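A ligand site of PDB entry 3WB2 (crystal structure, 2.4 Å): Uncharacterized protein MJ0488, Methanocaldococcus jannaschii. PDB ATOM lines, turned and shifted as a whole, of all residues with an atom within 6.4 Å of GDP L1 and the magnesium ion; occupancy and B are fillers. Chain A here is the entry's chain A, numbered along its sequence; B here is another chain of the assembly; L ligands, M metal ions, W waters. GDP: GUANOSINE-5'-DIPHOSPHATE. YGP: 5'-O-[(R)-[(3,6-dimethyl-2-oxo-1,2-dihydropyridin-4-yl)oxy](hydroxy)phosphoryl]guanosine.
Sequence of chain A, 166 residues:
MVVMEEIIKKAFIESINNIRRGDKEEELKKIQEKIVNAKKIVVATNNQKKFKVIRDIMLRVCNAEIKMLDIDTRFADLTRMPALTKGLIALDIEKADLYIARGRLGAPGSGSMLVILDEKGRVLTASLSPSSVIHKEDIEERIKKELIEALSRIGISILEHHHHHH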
ATOM      1  N   ALA A  44      14.815  -6.526 -27.572  1.00  0.00           N
ATOM      2  CA  ALA A  44      13.687  -5.639 -27.152  1.00  0.00           C
ATOM      3  C   ALA A  44      13.761  -5.393 -25.713  1.00  0.00           C
ATOM      4  O   ALA A  44      12.982  -5.946 -24.944  1.00  0.00           O
ATOM      5  CB  ALA A  44      12.344  -6.215 -27.482  1.00  0.00           C
ATOM      6  N   THR A  45      14.737  -4.583 -25.355  1.00  0.00           N
ATOM      7  CA  THR A  45      14.989  -4.198 -23.971  1.00  0.00           C
ATOM      8  C   THR A  45      15.515  -2.740 -23.985  1.00  0.00           C
ATOM      9  O   THR A  45      16.089  -2.280 -25.024  1.00  0.00           O
ATOM     10  CB  THR A  45      15.994  -5.176 -23.280  1.00  0.00           C
ATOM     11  OG1 THR A  45      16.056  -4.842 -21.910  1.00  0.00           O
ATOM     12  CG2 THR A  45      17.438  -5.073 -23.829  1.00  0.00           C
ATOM     13  N   ASN A  46      15.308  -2.038 -22.858  1.00  0.00           N
ATOM     14  CA  ASN A  46      16.006  -0.763 -22.579  1.00  0.00           C
ATOM     15  C   ASN A  46      17.061  -0.935 -21.472  1.00  0.00           C
ATOM     16  O   ASN A  46      17.703   0.023 -21.077  1.00  0.00           O
ATOM     17  CB  ASN A  46      15.053   0.376 -22.122  1.00  0.00           C
ATOM     18  CG  ASN A  46      13.803   0.526 -22.989  1.00  0.00           C
ATOM     19  OD1 ASN A  46      12.704   0.803 -22.452  1.00  0.00           O
ATOM     20  ND2 ASN A  46      13.954   0.380 -24.321  1.00  0.00           N
ATOM     21  N   ASN A  47      17.235  -2.138 -20.954  1.00  0.00           N
ATOM     22  CA  ASN A  47      18.214  -2.314 -19.907  1.00  0.00           C
ATOM     23  C   ASN A  47      19.589  -2.686 -20.460  1.00  0.00           C
ATOM     24  O   ASN A  47      19.802  -3.787 -21.004  1.00  0.00           O
ATOM     25  CB  ASN A  47      17.739  -3.381 -18.912  1.00  0.00           C
ATOM     26  CG  ASN A  47      18.658  -3.511 -17.706  1.00  0.00           C
ATOM     27  OD1 ASN A  47      18.616  -4.529 -17.016  1.00  0.00           O
ATOM     28  ND2 ASN A  47      19.484  -2.493 -17.442  1.00  0.00           N
ATOM     29  N   GLN A  48      20.531  -1.775 -20.276  1.00  0.00           N
ATOM     30  CA  GLN A  48      21.910  -1.982 -20.727  1.00  0.00           C
ATOM     31  C   GLN A  48      22.594  -3.218 -20.100  1.00  0.00           C
ATOM     32  O   GLN A  48      23.477  -3.832 -20.712  1.00  0.00           O
ATOM     33  CB  GLN A  48      22.676  -0.706 -20.484  1.00  0.00           C
ATOM     34  CG  GLN A  48      23.535  -0.270 -21.644  1.00  0.00           C
ATOM     35  CD  GLN A  48      24.929  -0.775 -21.423  1.00  0.00           C
ATOM     36  OE1 GLN A  48      25.529  -1.410 -22.297  1.00  0.00           O
ATOM     37  NE2 GLN A  48      25.450  -0.534 -20.218  1.00  0.00           N
ATOM     38  N   LYS A  49      22.162  -3.642 -18.908  1.00  0.00           N
ATOM     39  CA  LYS A  49      22.724  -4.860 -18.339  1.00  0.00           C
ATOM     40  C   LYS A  49      22.239  -6.118 -19.010  1.00  0.00           C
ATOM     41  O   LYS A  49      23.037  -7.046 -19.182  1.00  0.00           O
ATOM     42  CB  LYS A  49      22.396  -5.007 -16.857  1.00  0.00           C
ATOM     43  CG  LYS A  49      23.134  -4.063 -15.926  1.00  0.00           C
ATOM     44  CD  LYS A  49      22.955  -4.534 -14.511  1.00  0.00           C
ATOM     45  CE  LYS A  49      21.614  -4.123 -13.942  1.00  0.00           C
ATOM     46  NZ  LYS A  49      21.867  -3.792 -12.523  1.00  0.00           N
ATOM     47  N   LYS A  50      20.947  -6.221 -19.312  1.00  0.00           N
ATOM     48  CA  LYS A  50      20.461  -7.373 -20.054  1.00  0.00           C
ATOM     49  C   LYS A  50      21.108  -7.345 -21.430  1.00  0.00           C
ATOM     50  O   LYS A  50      21.606  -8.390 -21.885  1.00  0.00           O
ATOM     51  CB  LYS A  50      18.931  -7.411 -20.234  1.00  0.00           C
ATOM     52  CG  LYS A  50      18.025  -7.414 -18.999  1.00  0.00           C
ATOM     53  CD  LYS A  50      16.544  -7.449 -19.471  1.00  0.00           C
ATOM     54  CE  LYS A  50      15.593  -7.363 -18.279  1.00  0.00           C
ATOM     55  NZ  LYS A  50      14.129  -7.554 -18.556  1.00  0.00           N
ATOM     56  N   ASP A  72      10.496   3.431 -25.015  1.00  0.00           N
ATOM     57  CA  ASP A  72      10.187   2.855 -23.708  1.00  0.00           C
ATOM     58  C   ASP A  72       9.386   1.581 -23.851  1.00  0.00           C
ATOM     59  O   ASP A  72       8.331   1.589 -24.482  1.00  0.00           O
ATOM     60  CB  ASP A  72       9.342   3.828 -22.880  1.00  0.00           C
ATOM     61  CG  ASP A  72       9.431   3.557 -21.369  1.00  0.00           C
ATOM     62  OD1 ASP A  72       9.565   2.399 -20.893  1.00  0.00           O
ATOM     63  OD2 ASP A  72       9.386   4.545 -20.622  1.00  0.00           O
ATOM     64  N   THR A  73       9.879   0.525 -23.213  1.00  0.00           N
ATOM     65  CA  THR A  73       9.280  -0.823 -23.174  1.00  0.00           C
ATOM     66  C   THR A  73       8.366  -1.051 -21.932  1.00  0.00           C
ATOM     67  O   THR A  73       7.708  -2.080 -21.821  1.00  0.00           O
ATOM     68  CB  THR A  73      10.378  -1.955 -23.146  1.00  0.00           C
ATOM     69  OG1 THR A  73      11.238  -1.776 -21.982  1.00  0.00           O
ATOM     70  CG2 THR A  73      11.248  -2.029 -24.453  1.00  0.00           C
ATOM     71  N   ARG A  74       8.309  -0.127 -20.981  1.00  0.00           N
ATOM     72  CA  ARG A  74       7.582  -0.441 -19.773  1.00  0.00           C
ATOM     73  C   ARG A  74       6.076  -0.706 -19.935  1.00  0.00           C
ATOM     74  O   ARG A  74       5.455  -1.313 -19.055  1.00  0.00           O
ATOM     75  CB  ARG A  74       7.789   0.628 -18.720  1.00  0.00           C
ATOM     76  CG  ARG A  74       6.884   1.812 -18.861  1.00  0.00           C
ATOM     77  CD  ARG A  74       7.318   2.835 -17.834  1.00  0.00           C
ATOM     78  NE  ARG A  74       6.348   3.890 -17.638  1.00  0.00           N
ATOM     79  CZ  ARG A  74       6.492   5.102 -18.159  1.00  0.00           C
ATOM     80  NH1 ARG A  74       7.557   5.370 -18.884  1.00  0.00           N
ATOM     81  NH2 ARG A  74       5.594   6.047 -17.950  1.00  0.00           N
ATOM     82  N   ASP A  77       4.059  -4.202 -19.670  1.00  0.00           N
ATOM     83  CA  ASP A  77       3.720  -4.764 -18.387  1.00  0.00           C
ATOM     84  C   ASP A  77       2.212  -4.600 -18.078  1.00  0.00           C
ATOM     85  O   ASP A  77       1.777  -5.101 -17.071  1.00  0.00           O
ATOM     86  CB  ASP A  77       4.685  -4.253 -17.287  1.00  0.00           C
ATOM     87  CG  ASP A  77       6.179  -4.682 -17.519  1.00  0.00           C
ATOM     88  OD1 ASP A  77       6.450  -5.735 -18.180  1.00  0.00           O
ATOM     89  OD2 ASP A  77       7.101  -3.969 -17.030  1.00  0.00           O
ATOM     90  N   LYS A  86       6.662  -7.404 -25.907  1.00  0.00           N
ATOM     91  CA  LYS A  86       7.919  -6.707 -26.201  1.00  0.00           C
ATOM     92  C   LYS A  86       8.544  -7.148 -27.531  1.00  0.00           C
ATOM     93  O   LYS A  86       8.915  -6.308 -28.378  1.00  0.00           O
ATOM     94  CB  LYS A  86       8.926  -6.933 -25.083  1.00  0.00           C
ATOM     95  CG  LYS A  86       8.899  -5.900 -24.013  1.00  0.00           C
ATOM     96  CD  LYS A  86       9.911  -6.252 -22.912  1.00  0.00           C
ATOM     97  CE  LYS A  86       9.330  -6.000 -21.531  1.00  0.00           C
ATOM     98  NZ  LYS A  86      10.242  -6.680 -20.617  1.00  0.00           N
ATOM     99  N   ARG A 102      13.076 -10.199 -23.189  1.00  0.00           N
ATOM    100  CA  ARG A 102      12.971 -10.781 -21.836  1.00  0.00           C
ATOM    101  C   ARG A 102      12.125  -9.975 -20.866  1.00  0.00           C
ATOM    102  O   ARG A 102      12.488  -8.848 -20.528  1.00  0.00           O
ATOM    103  CB  ARG A 102      14.371 -10.999 -21.262  1.00  0.00           C
ATOM    104  CG  ARG A 102      14.452 -12.044 -20.132  1.00  0.00           C
ATOM    105  CD  ARG A 102      14.315 -11.410 -18.750  1.00  0.00           C
ATOM    106  NE  ARG A 102      14.676 -12.358 -17.712  1.00  0.00           N
ATOM    107  CZ  ARG A 102      14.779 -12.045 -16.425  1.00  0.00           C
ATOM    108  NH1 ARG A 102      15.145 -12.978 -15.561  1.00  0.00           N
ATOM    109  NH2 ARG A 102      14.542 -10.804 -16.008  1.00  0.00           N
ATOM    110  N   GLY A 103      11.026 -10.548 -20.363  1.00  0.00           N
ATOM    111  CA  GLY A 103      10.154  -9.906 -19.359  1.00  0.00           C
ATOM    112  C   GLY A 103       9.354 -10.872 -18.475  1.00  0.00           C
ATOM    113  O   GLY A 103       9.712 -12.061 -18.347  1.00  0.00           O
ATOM    114  N   ILE A 139      20.726 -10.556 -11.669  1.00  0.00           N
ATOM    115  CA  ILE A 139      20.078 -10.617 -12.964  1.00  0.00           C
ATOM    116  C   ILE A 139      20.953 -11.124 -14.151  1.00  0.00           C
ATOM    117  O   ILE A 139      20.450 -11.895 -15.013  1.00  0.00           O
ATOM    118  CB  ILE A 139      19.291  -9.323 -13.312  1.00  0.00           C
ATOM    119  CG1 ILE A 139      18.207  -9.651 -14.368  1.00  0.00           C
ATOM    120  CG2 ILE A 139      20.237  -8.187 -13.712  1.00  0.00           C
ATOM    121  CD1 ILE A 139      17.304  -8.490 -14.738  1.00  0.00           C
ATOM    122  N   ASN B  18       6.314   4.045 -13.659  1.00  0.00           N
ATOM    123  CA  ASN B  18       7.683   3.635 -13.874  1.00  0.00           C
ATOM    124  C   ASN B  18       8.464   3.310 -12.596  1.00  0.00           C
ATOM    125  O   ASN B  18       9.660   3.523 -12.556  1.00  0.00           O
ATOM    126  CB  ASN B  18       8.425   4.687 -14.734  1.00  0.00           C
ATOM    127  CG  ASN B  18       9.757   4.185 -15.278  1.00  0.00           C
ATOM    128  OD1 ASN B  18       9.954   2.990 -15.508  1.00  0.00           O
ATOM    129  ND2 ASN B  18      10.689   5.082 -15.460  1.00  0.00           N
ATOM    130  N   ARG B  20       7.850  -0.015 -11.032  1.00  0.00           N
ATOM    131  CA  ARG B  20       7.808  -1.472 -10.890  1.00  0.00           C
ATOM    132  C   ARG B  20       9.219  -2.117 -10.958  1.00  0.00           C
ATOM    133  O   ARG B  20      10.050  -1.726 -11.810  1.00  0.00           O
ATOM    134  CB  ARG B  20       6.915  -2.057 -11.989  1.00  0.00           C
ATOM    135  CG  ARG B  20       6.720  -3.559 -11.958  1.00  0.00           C
ATOM    136  CD  ARG B  20       5.826  -4.030 -10.828  1.00  0.00           C
ATOM    137  NE  ARG B  20       5.692  -5.471 -10.924  1.00  0.00           N
ATOM    138  CZ  ARG B  20       4.992  -6.272 -10.118  1.00  0.00           C
ATOM    139  NH1 ARG B  20       4.302  -5.786  -9.080  1.00  0.00           N
ATOM    140  NH2 ARG B  20       4.993  -7.582 -10.395  1.00  0.00           N
ATOM    141  N   ARG B  21       9.462  -3.098 -10.104  1.00  0.00           N
ATOM    142  CA  ARG B  21      10.652  -3.952 -10.282  1.00  0.00           C
ATOM    143  C   ARG B  21      10.271  -5.370 -10.713  1.00  0.00           C
ATOM    144  O   ARG B  21       9.707  -5.553 -11.808  1.00  0.00           O
ATOM    145  CB  ARG B  21      11.515  -3.986  -9.012  1.00  0.00           C
ATOM    146  CG  ARG B  21      12.149  -2.641  -8.729  1.00  0.00           C
ATOM    147  CD  ARG B  21      13.192  -2.243  -9.783  1.00  0.00           C
ATOM    148  NE  ARG B  21      13.683  -0.872  -9.561  1.00  0.00           N
ATOM    149  CZ  ARG B  21      13.523   0.149 -10.410  1.00  0.00           C
ATOM    150  NH1 ARG B  21      14.000   1.336 -10.094  1.00  0.00           N
ATOM    151  NH2 ARG B  21      12.901  -0.020 -11.577  1.00  0.00           N
HETATM  152  PB  GDP L   1      13.349  -4.003 -20.305  1.00  0.00           P
HETATM  153  O1B GDP L   1      13.608  -3.009 -21.437  1.00  0.00           O
HETATM  154  O2B GDP L   1      13.917  -5.403 -20.482  1.00  0.00           O
HETATM  155  O3B GDP L   1      11.895  -3.995 -19.797  1.00  0.00           O
HETATM  156  O3A GDP L   1      14.310  -3.405 -19.128  1.00  0.00           O
HETATM  157  PA  GDP L   1      14.054  -3.425 -17.518  1.00  0.00           P
HETATM  158  O1A GDP L   1      12.649  -2.959 -17.201  1.00  0.00           O
HETATM  159  O2A GDP L   1      14.641  -4.683 -16.867  1.00  0.00           O
HETATM  160  O5' GDP L   1      15.039  -2.214 -17.143  1.00  0.00           O
HETATM  161  C5' GDP L   1      14.622  -0.844 -17.359  1.00  0.00           C
HETATM  162  C4' GDP L   1      15.450   0.181 -16.582  1.00  0.00           C
HETATM  163  O4' GDP L   1      14.870   0.356 -15.270  1.00  0.00           O
HETATM  164  C3' GDP L   1      16.946  -0.152 -16.348  1.00  0.00           C
HETATM  165  O3' GDP L   1      17.846   0.024 -17.464  1.00  0.00           O
HETATM  166  C2' GDP L   1      17.242   0.683 -15.122  1.00  0.00           C
HETATM  167  O2' GDP L   1      17.540   2.030 -15.475  1.00  0.00           O
HETATM  168  C1' GDP L   1      15.912   0.691 -14.349  1.00  0.00           C
HETATM  169  N9  GDP L   1      16.091  -0.347 -13.307  1.00  0.00           N
HETATM  170  C8  GDP L   1      15.727  -1.652 -13.387  1.00  0.00           C
HETATM  171  N7  GDP L   1      16.094  -2.341 -12.278  1.00  0.00           N
HETATM  172  C5  GDP L   1      16.733  -1.455 -11.467  1.00  0.00           C
HETATM  173  C6  GDP L   1      17.381  -1.496 -10.113  1.00  0.00           C
HETATM  174  O6  GDP L   1      17.423  -2.555  -9.436  1.00  0.00           O
HETATM  175  N1  GDP L   1      17.916  -0.358  -9.639  1.00  0.00           N
HETATM  176  C2  GDP L   1      17.892   0.815 -10.321  1.00  0.00           C
HETATM  177  N2  GDP L   1      18.469   1.901  -9.740  1.00  0.00           N
HETATM  178  N3  GDP L   1      17.318   0.933 -11.561  1.00  0.00           N
HETATM  179  C4  GDP L   1      16.740  -0.149 -12.156  1.00  0.00           C
HETATM  180  C2  YGP L   2      17.407 -10.125  -9.792  1.00  0.00           C
HETATM  181  N2  YGP L   2      18.327  -9.879  -8.858  1.00  0.00           N
HETATM  182  C4  YGP L   2      15.594  -9.354 -11.097  1.00  0.00           C
HETATM  183  C5  YGP L   2      15.481 -10.570 -11.713  1.00  0.00           C
HETATM  184  C6  YGP L   2      16.326 -11.621 -11.408  1.00  0.00           C
HETATM  185  O6  YGP L   2      16.225 -12.745 -11.946  1.00  0.00           O
HETATM  186  N1  YGP L   2      17.334 -11.414 -10.420  1.00  0.00           N
HETATM  187  N3  YGP L   2      16.552  -9.143 -10.147  1.00  0.00           N
HETATM  188  N7  YGP L   2      14.477 -10.482 -12.606  1.00  0.00           N
HETATM  189  C8  YGP L   2      13.983  -9.243 -12.507  1.00  0.00           C
HETATM  190  N9  YGP L   2      14.661  -8.513 -11.598  1.00  0.00           N
HETATM  191  C1' YGP L   2      14.315  -7.060 -11.255  1.00  0.00           C
HETATM  192  O4' YGP L   2      12.946  -6.689 -11.719  1.00  0.00           O
HETATM  193  C2' YGP L   2      15.185  -5.983 -11.911  1.00  0.00           C
HETATM  194  O2' YGP L   2      14.993  -4.718 -11.201  1.00  0.00           O
HETATM  195  C3' YGP L   2      14.520  -5.895 -13.301  1.00  0.00           C
HETATM  196  O3' YGP L   2      15.019  -4.790 -14.109  1.00  0.00           O
HETATM  197  C4' YGP L   2      13.044  -5.753 -12.905  1.00  0.00           C
HETATM  198  C5' YGP L   2      12.127  -6.122 -14.099  1.00  0.00           C
HETATM  199  O5' YGP L   2      12.520  -7.423 -14.690  1.00  0.00           O
HETATM  200  PBG YGP L   2      11.780  -7.933 -16.135  1.00  0.00           P
HETATM  201  OAI YGP L   2      12.226  -9.506 -16.456  1.00  0.00           O
HETATM  202  OAF YGP L   2      12.002  -7.034 -17.314  1.00  0.00           O
HETATM  203  OAR YGP L   2      10.171  -7.962 -15.764  1.00  0.00           O
HETATM  204  CAW YGP L   2       9.492  -8.603 -14.741  1.00  0.00           C
HETATM  205  CAK YGP L   2       9.815  -9.890 -14.224  1.00  0.00           C
HETATM  206  CAT YGP L   2       9.020 -10.454 -13.212  1.00  0.00           C
HETATM  207  CAA YGP L   2       9.299 -11.739 -12.654  1.00  0.00           C
HETATM  208  NAO YGP L   2       7.900  -9.722 -12.744  1.00  0.00           N
HETATM  209  CAX YGP L   2       7.560  -8.441 -13.261  1.00  0.00           C
HETATM  210  OAD YGP L   2       6.566  -7.846 -12.815  1.00  0.00           O
HETATM  211  CAV YGP L   2       8.392  -7.878 -14.269  1.00  0.00           C
HETATM  212  CAB YGP L   2       8.131  -6.605 -14.840  1.00  0.00           C
HETATM  213 MG    MG M   1      10.638  -3.132 -18.306  1.00  0.00          MG
HETATM  214  O   HOH W   1      17.888  -4.383 -13.550  1.00  0.00           O
HETATM  215  O   HOH W   2      10.249  -4.964 -17.119  1.00  0.00           O
HETATM  216  O   HOH W   3      11.996  -2.125 -14.275  1.00  0.00           O
HETATM  217  O   HOH W   4      20.337   0.697 -19.616  1.00  0.00           O
HETATM  218  O   HOH W   5      11.283  -1.497 -19.582  1.00  0.00           O
HETATM  219  O   HOH W   6       8.783  -3.725 -19.336  1.00  0.00           O
HETATM  220  O   HOH W   7       9.707  -2.130 -16.638  1.00  0.00           O
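N of Asn 46 lies within hydrogen-bond range of O1B of GDP L1 (2.4 Å).
The side-chain hydroxyl (OG1) of Thr 45 is in hydrogen-bond range of an oxygen (O2B) of GDP L1 (2.6 Å).
OG1 of Thr 73 lies within hydrogen-bond range of O1B of GDP L1 (2.7 Å).
The side-chain amino group (NZ) of Lys 50 lies within salt-bridge range of an oxygen (O2B) of GDP L1 (2.9 Å).
The side-chain amide nitrogen (ND2) of Asn 47 lies within hydrogen-bond range of an oxygen (O3') of GDP L1, 3.0 Å away.
O2B of GDP L1 is in salt-bridge range of NZ of Lys 86 (3.9 Å).
NZ of Lys 50 lies within salt-bridge range of OAF of YGP L2 (2.5 Å).
OAF of YGP L2 is in salt-bridge range of NZ of Lys 86 (3.8 Å).
The guanidinium group (NH2) of Arg 102 is in salt-bridge range of an oxygen (OAI) of YGP L2, 2.7 Å away.
The guanidinium group (NH2) of Arg 20 of chain B is in hydrogen-bond range of an oxygen (OAD) of YGP L2 (2.9 Å).
An oxygen (O3') of YGP L2 is in hydrogen-bond range of an oxygen (O2A) of GDP L1 (2.8 Å).
The side-chain amide oxygen (OD1) of Asn 46 is in hydrogen-bond range of the backbone NH (N) of Thr 73 (2.9 Å).
The side-chain hydroxyl of Thr 45 sits at hydrogen-bond distance from the backbone NH of Asn 47.
O of Arg 102 lies within hydrogen-bond range of NZ of Lys 50 (2.9 Å).
ND2 of Asn 47 sits close to N of Lys 49, at 3.3 Å.
The side-chain amino group (NZ) of Lys 86 sits at hydrogen-bond distance from the backbone carbonyl oxygen (O) of Arg 102.
Arg 102 touches GDP L1 (O to O2B, 3.7 Å).
Arg 21 of chain B touches GDP L1.
Within 4 Å of GDP L1: Thr 45, Asn 46, Asn 47, Lys 50, Thr 73, Lys 86, Arg 102 and Arg 21 of chain B.
Thr 73 touches the magnesium ion.
Asp 77 touches the magnesium ion.
Of the 18 residues printed, 2 come within 4 Å of the magnesium ion.
The nearest printed residue that does not touch the magnesium ion is Lys 86 (4.3 Å).
The magnesium ion is bound by an oxygen (O3B) of GDP L1 (2.1 Å), water W7 (2.2 Å), water W5 (2.2 Å), water W6 (2.2 Å), water W2 (2.2 Å) and an oxygen (O1A) of GDP L1 (2.3 Å).
Water W2 lies within hydrogen-bond range of OAF of YGP L2 (2.7 Å) and OD2 of Asp 77 (3.3 Å).
Water W6 lies within hydrogen-bond range of the side-chain carboxylate (OD2) of Asp 77 and the backbone carbonyl oxygen (O) of Thr 73.
Water W5 bridges the side-chain hydroxyl of Thr 73 (2.4 Å) and an oxygen (O1B) of GDP L1 (3.3 Å).
Water W1 lies within hydrogen-bond range of O3' of YGP L2 (3.0 Å) and N7 of GDP L1 (3.0 Å).
Water W4 lies within hydrogen-bond range of the backbone NH (N) of Gln 48, the backbone carbonyl oxygen (O) of Asn 46 and an oxygen (O3') of GDP L1.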
